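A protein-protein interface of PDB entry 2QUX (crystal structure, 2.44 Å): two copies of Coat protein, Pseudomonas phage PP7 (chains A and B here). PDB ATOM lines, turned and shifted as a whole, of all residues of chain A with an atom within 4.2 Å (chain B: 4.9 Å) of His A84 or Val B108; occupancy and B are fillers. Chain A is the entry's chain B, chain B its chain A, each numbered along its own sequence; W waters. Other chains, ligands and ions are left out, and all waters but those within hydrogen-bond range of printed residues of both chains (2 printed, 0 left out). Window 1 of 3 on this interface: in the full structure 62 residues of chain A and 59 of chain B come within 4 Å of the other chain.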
ATOM      1  N   VAL A  59      20.670  15.430  26.721  1.00  0.00           N
ATOM      2  CA  VAL A  59      20.693  16.571  25.827  1.00  0.00           C
ATOM      3  C   VAL A  59      19.995  17.698  26.560  1.00  0.00           C
ATOM      4  O   VAL A  59      18.866  17.530  27.010  1.00  0.00           O
ATOM      5  CB  VAL A  59      19.928  16.272  24.514  1.00  0.00           C
ATOM      6  CG1 VAL A  59      19.832  17.492  23.611  1.00  0.00           C
ATOM      7  CG2 VAL A  59      20.544  15.125  23.826  1.00  0.00           C
ATOM      8  N   ASN A  60      20.681  18.829  26.692  1.00  0.00           N
ATOM      9  CA  ASN A  60      20.103  20.050  27.225  1.00  0.00           C
ATOM     10  C   ASN A  60      20.002  21.091  26.107  1.00  0.00           C
ATOM     11  O   ASN A  60      20.936  21.287  25.348  1.00  0.00           O
ATOM     12  CB  ASN A  60      20.903  20.546  28.440  1.00  0.00           C
ATOM     13  CG  ASN A  60      20.906  19.524  29.600  1.00  0.00           C
ATOM     14  OD1 ASN A  60      21.958  19.018  29.998  1.00  0.00           O
ATOM     15  ND2 ASN A  60      19.731  19.199  30.109  1.00  0.00           N
ATOM     16  N   LEU A  61      18.826  21.688  25.973  1.00  0.00           N
ATOM     17  CA  LEU A  61      18.571  22.755  25.027  1.00  0.00           C
ATOM     18  C   LEU A  61      17.901  23.855  25.819  1.00  0.00           C
ATOM     19  O   LEU A  61      16.911  23.584  26.478  1.00  0.00           O
ATOM     20  CB  LEU A  61      17.600  22.271  23.957  1.00  0.00           C
ATOM     21  CG  LEU A  61      18.059  21.895  22.573  1.00  0.00           C
ATOM     22  CD1 LEU A  61      19.212  20.941  22.614  1.00  0.00           C
ATOM     23  CD2 LEU A  61      16.833  21.275  21.896  1.00  0.00           C
ATOM     24  N   TRP A  82      12.919  28.689  28.123  1.00  0.00           N
ATOM     25  CA  TRP A  82      12.290  27.391  27.889  1.00  0.00           C
ATOM     26  C   TRP A  82      13.438  26.453  27.630  1.00  0.00           C
ATOM     27  O   TRP A  82      14.153  26.594  26.645  1.00  0.00           O
ATOM     28  CB  TRP A  82      11.333  27.437  26.686  1.00  0.00           C
ATOM     29  CG  TRP A  82      10.433  26.239  26.578  1.00  0.00           C
ATOM     30  CD1 TRP A  82      10.764  24.936  26.791  1.00  0.00           C
ATOM     31  CD2 TRP A  82       9.052  26.238  26.192  1.00  0.00           C
ATOM     32  NE1 TRP A  82       9.688  24.133  26.592  1.00  0.00           N
ATOM     33  CE2 TRP A  82       8.618  24.896  26.218  1.00  0.00           C
ATOM     34  CE3 TRP A  82       8.149  27.233  25.808  1.00  0.00           C
ATOM     35  CZ2 TRP A  82       7.311  24.519  25.894  1.00  0.00           C
ATOM     36  CZ3 TRP A  82       6.835  26.857  25.505  1.00  0.00           C
ATOM     37  CH2 TRP A  82       6.437  25.514  25.541  1.00  0.00           C
ATOM     38  N   SER A  83      13.606  25.496  28.528  1.00  0.00           N
ATOM     39  CA  SER A  83      14.726  24.600  28.478  1.00  0.00           C
ATOM     40  C   SER A  83      14.178  23.201  28.448  1.00  0.00           C
ATOM     41  O   SER A  83      13.040  22.972  28.845  1.00  0.00           O
ATOM     42  CB  SER A  83      15.666  24.836  29.644  1.00  0.00           C
ATOM     43  OG  SER A  83      15.097  24.413  30.841  1.00  0.00           O
ATOM     44  N   HIS A  84      14.967  22.307  27.888  1.00  0.00           N
ATOM     45  CA  HIS A  84      14.567  20.946  27.566  1.00  0.00           C
ATOM     46  C   HIS A  84      15.653  20.073  28.133  1.00  0.00           C
ATOM     47  O   HIS A  84      16.830  20.430  28.077  1.00  0.00           O
ATOM     48  CB  HIS A  84      14.569  20.755  26.067  1.00  0.00           C
ATOM     49  CG  HIS A  84      13.678  21.709  25.341  1.00  0.00           C
ATOM     50  ND1 HIS A  84      12.409  21.373  24.931  1.00  0.00           N
ATOM     51  CD2 HIS A  84      13.869  22.991  24.962  1.00  0.00           C
ATOM     52  CE1 HIS A  84      11.857  22.404  24.320  1.00  0.00           C
ATOM     53  NE2 HIS A  84      12.725  23.398  24.321  1.00  0.00           N
ATOM     54  N   ASP A  85      15.257  18.934  28.673  1.00  0.00           N
ATOM     55  CA  ASP A  85      16.180  17.966  29.175  1.00  0.00           C
ATOM     56  C   ASP A  85      15.743  16.586  28.661  1.00  0.00           C
ATOM     57  O   ASP A  85      14.697  16.041  29.056  1.00  0.00           O
ATOM     58  CB  ASP A  85      16.158  18.073  30.697  1.00  0.00           C
ATOM     59  CG  ASP A  85      17.219  17.270  31.362  1.00  0.00           C
ATOM     60  OD1 ASP A  85      17.362  17.472  32.587  1.00  0.00           O
ATOM     61  OD2 ASP A  85      17.887  16.429  30.703  1.00  0.00           O
ATOM     62  N   VAL A  86      16.570  16.016  27.789  1.00  0.00           N
ATOM     63  CA  VAL A  86      16.224  14.795  27.104  1.00  0.00           C
ATOM     64  C   VAL A  86      17.152  13.674  27.524  1.00  0.00           C
ATOM     65  O   VAL A  86      18.356  13.809  27.425  1.00  0.00           O
ATOM     66  CB  VAL A  86      16.250  14.982  25.583  1.00  0.00           C
ATOM     67  CG1 VAL A  86      15.564  13.812  24.914  1.00  0.00           C
ATOM     68  CG2 VAL A  86      15.589  16.306  25.230  1.00  0.00           C
ATOM     69  N   TYR A 101      10.743  11.967  20.250  1.00  0.00           N
ATOM     70  CA  TYR A 101      10.831  13.196  19.455  1.00  0.00           C
ATOM     71  C   TYR A 101       9.450  13.614  18.935  1.00  0.00           C
ATOM     72  O   TYR A 101       9.008  14.716  19.202  1.00  0.00           O
ATOM     73  CB  TYR A 101      11.854  13.093  18.282  1.00  0.00           C
ATOM     74  CG  TYR A 101      11.822  14.338  17.422  1.00  0.00           C
ATOM     75  CD1 TYR A 101      12.396  15.519  17.872  1.00  0.00           C
ATOM     76  CD2 TYR A 101      11.112  14.372  16.219  1.00  0.00           C
ATOM     77  CE1 TYR A 101      12.317  16.690  17.126  1.00  0.00           C
ATOM     78  CE2 TYR A 101      11.028  15.545  15.461  1.00  0.00           C
ATOM     79  CZ  TYR A 101      11.618  16.699  15.926  1.00  0.00           C
ATOM     80  OH  TYR A 101      11.531  17.848  15.185  1.00  0.00           O
ATOM     81  N   LYS A 105       7.238  16.890  19.815  1.00  0.00           N
ATOM     82  CA  LYS A 105       6.906  17.793  18.696  1.00  0.00           C
ATOM     83  C   LYS A 105       5.399  18.131  18.748  1.00  0.00           C
ATOM     84  O   LYS A 105       5.007  19.293  18.821  1.00  0.00           O
ATOM     85  CB  LYS A 105       7.276  17.151  17.334  1.00  0.00           C
ATOM     86  CG  LYS A 105       7.526  18.152  16.218  1.00  0.00           C
ATOM     87  CD  LYS A 105       7.323  17.660  14.738  1.00  0.00           C
ATOM     88  CE  LYS A 105       7.673  16.200  14.439  1.00  0.00           C
ATOM     89  NZ  LYS A 105       8.223  15.990  13.043  1.00  0.00           N
ATOM     90  N   TRP B  82      11.678  13.333  28.042  1.00  0.00           N
ATOM     91  CA  TRP B  82      11.862  14.681  27.545  1.00  0.00           C
ATOM     92  C   TRP B  82      11.075  15.619  28.468  1.00  0.00           C
ATOM     93  O   TRP B  82       9.855  15.640  28.442  1.00  0.00           O
ATOM     94  CB  TRP B  82      11.394  14.762  26.098  1.00  0.00           C
ATOM     95  CG  TRP B  82      11.801  15.976  25.390  1.00  0.00           C
ATOM     96  CD1 TRP B  82      11.842  17.250  25.879  1.00  0.00           C
ATOM     97  CD2 TRP B  82      12.214  16.059  24.035  1.00  0.00           C
ATOM     98  NE1 TRP B  82      12.239  18.106  24.921  1.00  0.00           N
ATOM     99  CE2 TRP B  82      12.483  17.412  23.770  1.00  0.00           C
ATOM    100  CE3 TRP B  82      12.381  15.121  23.007  1.00  0.00           C
ATOM    101  CZ2 TRP B  82      12.902  17.862  22.518  1.00  0.00           C
ATOM    102  CZ3 TRP B  82      12.786  15.566  21.773  1.00  0.00           C
ATOM    103  CH2 TRP B  82      13.061  16.922  21.537  1.00  0.00           C
ATOM    104  N   SER B  83      11.792  16.386  29.288  1.00  0.00           N
ATOM    105  CA  SER B  83      11.170  17.361  30.158  1.00  0.00           C
ATOM    106  C   SER B  83      11.388  18.776  29.662  1.00  0.00           C
ATOM    107  O   SER B  83      12.261  19.034  28.845  1.00  0.00           O
ATOM    108  CB  SER B  83      11.581  17.188  31.635  1.00  0.00           C
ATOM    109  OG  SER B  83      12.921  17.559  31.898  1.00  0.00           O
ATOM    110  N   HIS B  84      10.555  19.676  30.171  1.00  0.00           N
ATOM    111  CA  HIS B  84      10.508  21.071  29.758  1.00  0.00           C
ATOM    112  C   HIS B  84      10.494  21.893  31.018  1.00  0.00           C
ATOM    113  O   HIS B  84       9.823  21.525  31.982  1.00  0.00           O
ATOM    114  CB  HIS B  84       9.213  21.354  28.995  1.00  0.00           C
ATOM    115  CG  HIS B  84       9.008  20.461  27.810  1.00  0.00           C
ATOM    116  ND1 HIS B  84       9.262  20.867  26.522  1.00  0.00           N
ATOM    117  CD2 HIS B  84       8.610  19.170  27.724  1.00  0.00           C
ATOM    118  CE1 HIS B  84       9.013  19.875  25.689  1.00  0.00           C
ATOM    119  NE2 HIS B  84       8.616  18.831  26.394  1.00  0.00           N
ATOM    120  N   THR B 104       9.801  28.079  20.505  1.00  0.00           N
ATOM    121  CA  THR B 104      10.042  26.706  20.964  1.00  0.00           C
ATOM    122  C   THR B 104       9.359  25.645  20.123  1.00  0.00           C
ATOM    123  O   THR B 104       9.918  24.562  19.906  1.00  0.00           O
ATOM    124  CB  THR B 104       9.610  26.535  22.440  1.00  0.00           C
ATOM    125  OG1 THR B 104      10.324  27.480  23.235  1.00  0.00           O
ATOM    126  CG2 THR B 104       9.927  25.124  22.948  1.00  0.00           C
ATOM    127  N   LYS B 105       8.132  25.935  19.708  1.00  0.00           N
ATOM    128  CA  LYS B 105       7.378  25.071  18.804  1.00  0.00           C
ATOM    129  C   LYS B 105       8.171  24.881  17.490  1.00  0.00           C
ATOM    130  O   LYS B 105       8.352  23.760  16.983  1.00  0.00           O
ATOM    131  CB  LYS B 105       6.008  25.708  18.567  1.00  0.00           C
ATOM    132  CG  LYS B 105       5.030  24.923  17.677  1.00  0.00           C
ATOM    133  CD  LYS B 105       3.764  25.716  17.536  1.00  0.00           C
ATOM    134  CE  LYS B 105       2.785  25.149  16.521  1.00  0.00           C
ATOM    135  NZ  LYS B 105       1.541  25.990  16.495  1.00  0.00           N
ATOM    136  N   SER B 106       8.679  25.981  16.969  1.00  0.00           N
ATOM    137  CA  SER B 106       9.562  25.936  15.799  1.00  0.00           C
ATOM    138  C   SER B 106      10.858  25.171  16.049  1.00  0.00           C
ATOM    139  O   SER B 106      11.226  24.328  15.248  1.00  0.00           O
ATOM    140  CB  SER B 106       9.851  27.349  15.302  1.00  0.00           C
ATOM    141  OG  SER B 106      10.780  27.300  14.251  1.00  0.00           O
ATOM    142  N   LEU B 107      11.516  25.445  17.185  1.00  0.00           N
ATOM    143  CA  LEU B 107      12.786  24.798  17.551  1.00  0.00           C
ATOM    144  C   LEU B 107      12.683  23.286  17.588  1.00  0.00           C
ATOM    145  O   LEU B 107      13.451  22.573  16.950  1.00  0.00           O
ATOM    146  CB  LEU B 107      13.252  25.298  18.915  1.00  0.00           C
ATOM    147  CG  LEU B 107      14.554  24.782  19.526  1.00  0.00           C
ATOM    148  CD1 LEU B 107      15.742  25.152  18.663  1.00  0.00           C
ATOM    149  CD2 LEU B 107      14.688  25.342  20.941  1.00  0.00           C
ATOM    150  N   VAL B 108      11.732  22.809  18.365  1.00  0.00           N
ATOM    151  CA  VAL B 108      11.502  21.391  18.501  1.00  0.00           C
ATOM    152  C   VAL B 108      11.132  20.775  17.144  1.00  0.00           C
ATOM    153  O   VAL B 108      11.560  19.666  16.861  1.00  0.00           O
ATOM    154  CB  VAL B 108      10.407  21.099  19.562  1.00  0.00           C
ATOM    155  CG1 VAL B 108      10.073  19.631  19.591  1.00  0.00           C
ATOM    156  CG2 VAL B 108      10.866  21.569  20.954  1.00  0.00           C
ATOM    157  N   ALA B 109      10.389  21.507  16.301  1.00  0.00           N
ATOM    158  CA  ALA B 109       9.985  21.006  14.967  1.00  0.00           C
ATOM    159  C   ALA B 109      11.114  20.893  13.934  1.00  0.00           C
ATOM    160  O   ALA B 109      10.920  20.238  12.908  1.00  0.00           O
ATOM    161  CB  ALA B 109       8.833  21.848  14.383  1.00  0.00           C
ATOM    162  N   THR B 110      12.261  21.527  14.180  1.00  0.00           N
ATOM    163  CA  THR B 110      13.373  21.479  13.259  1.00  0.00           C
ATOM    164  C   THR B 110      14.009  20.082  13.150  1.00  0.00           C
ATOM    165  O   THR B 110      14.013  19.310  14.102  1.00  0.00           O
ATOM    166  CB  THR B 110      14.497  22.479  13.607  1.00  0.00           C
ATOM    167  OG1 THR B 110      15.118  22.108  14.840  1.00  0.00           O
ATOM    168  CG2 THR B 110      14.002  23.945  13.600  1.00  0.00           C
ATOM    169  N   VAL B 113      17.115  19.547  15.516  1.00  0.00           N
ATOM    170  CA  VAL B 113      16.768  19.000  16.840  1.00  0.00           C
ATOM    171  C   VAL B 113      16.366  17.534  16.774  1.00  0.00           C
ATOM    172  O   VAL B 113      16.639  16.789  17.711  1.00  0.00           O
ATOM    173  CB  VAL B 113      15.671  19.828  17.566  1.00  0.00           C
ATOM    174  CG1 VAL B 113      15.236  19.159  18.877  1.00  0.00           C
ATOM    175  CG2 VAL B 113      16.174  21.220  17.865  1.00  0.00           C
HETATM  176  O   HOH W   1      12.773  26.196  23.713  1.00  0.00           O
HETATM  177  O   HOH W   2       6.566  21.538  17.508  1.00  0.00           O
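The indole nitrogen of Trp B82 lies within hydrogen-bond range of a ring nitrogen (ND1) of His A84 (3.3 Å). O of Thr B110 sits at hydrogen-bond distance from OH of Tyr A101, at 3.1 Å. A ring nitrogen (ND1) of His B84 sits at hydrogen-bond distance from the indole nitrogen of Trp A82, at 3.3 Å. O of Val B108 lies within hydrogen-bond range of OH of Tyr A101. The backbone carbonyl oxygen (O) of Asp A85 lies within hydrogen-bond range of the backbone NH (N) of Ser B83 (2.9 Å). The backbone carbonyl oxygen (O) of Ala B109 sits close to the side-chain hydroxyl (OH) of Tyr A101, at 3.4 Å.
The backbone NH (N) of Val B113 lies within hydrogen-bond range of the side-chain hydroxyl (OG1) of Thr B110 (3.3 Å). The backbone carbonyl oxygen (O) of Leu B107 is in hydrogen-bond range of the side-chain hydroxyl (OG1) of Thr B110. The backbone carbonyl oxygen (O) of Val A59 sits at hydrogen-bond distance from the backbone NH (N) of Val A86, at 2.9 Å. The side-chain amide nitrogen (ND2) of Asn A60 sits at hydrogen-bond distance from the side-chain carboxylate (OD2) of Asp A85, at 3.4 Å. The backbone NH (N) of His A84 is in hydrogen-bond range of the backbone carbonyl oxygen (O) of Leu A61 (2.7 Å).
Among the printed residues, pairs that only touch across the chains: His A84 with Ser B83 (3.3 Å), Ser A83 with His B84 (3.3 Å), Trp A82 with Thr B104 (3.4 Å), Asp A85 with Trp B82 (3.5 Å), His A84 with His B84 (3.6 Å), His A84 with Thr B104 (3.6 Å), Val A86 with Trp B82 (3.6 Å), His A84 with Val B108 (3.6 Å), Lys A105 with Val B108 (3.8 Å), Tyr A101 with Trp B82 (3.8 Å) and Lys A105 with Ala B109 (3.97 Å).
Val A59 touches none of the printed residues of chain B. Of the printed residues of chain B, Ser A83 touches His B84. His A84 touches just these residues of chain B: Trp B82, Ser B83, His B84, Thr B104 and Val B108. Of the printed residues of chain A, His B84 touches Trp A82, Ser A83 and His A84. Val B108 touches just these residues of chain A: His A84 (3.6 Å), Tyr A101 (2.5 Å) and Lys A105 (3.8 Å). The nearest residue of chain B that does not touch His A84 is Leu B107 (4.4 Å). The nearest printed residue of chain A that does not touch Val B108 is Leu A61 (6.0 Å). The nearest printed residue of chain B that does not touch Ser A83 is Ser B83 (4.01 Å).
Hydrophobic or aromatic side chains of chain A that line the printed part of chain B: Trp A82, His A84, Val A86 and Tyr A101. Printed residues of chain B that touch a printed residue of chain A: Trp B82, Ser B83, His B84, Thr B104, Val B108, Ala B109 and Thr B110. Along chain B the printed residues that touch a printed residue of chain A span positions 82 to 110. Among the printed residues, no Asp or Glu carboxylate lies within 4 Å of a Lys or Arg side-chain nitrogen of the other chain.
Trp A82 touches His B84, and with the chains exchanged His A84 touches Trp B82. Ser A83 touches His B84, and with the chains exchanged His A84 touches Ser B83. His B84 touches its own counterpart, His A84. Positions printed for both chains: 82, 83, 84 and 105.
Water W1 lies within hydrogen-bond range of OG1 of Thr B104 (2.8 Å), NE2 of His A84 (2.9 Å) and O of Trp A82 (3.3 Å). Water W2 lies within hydrogen-bond range of O of Lys B105 (2.9 Å) and O of Lys A105 (3.0 Å).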
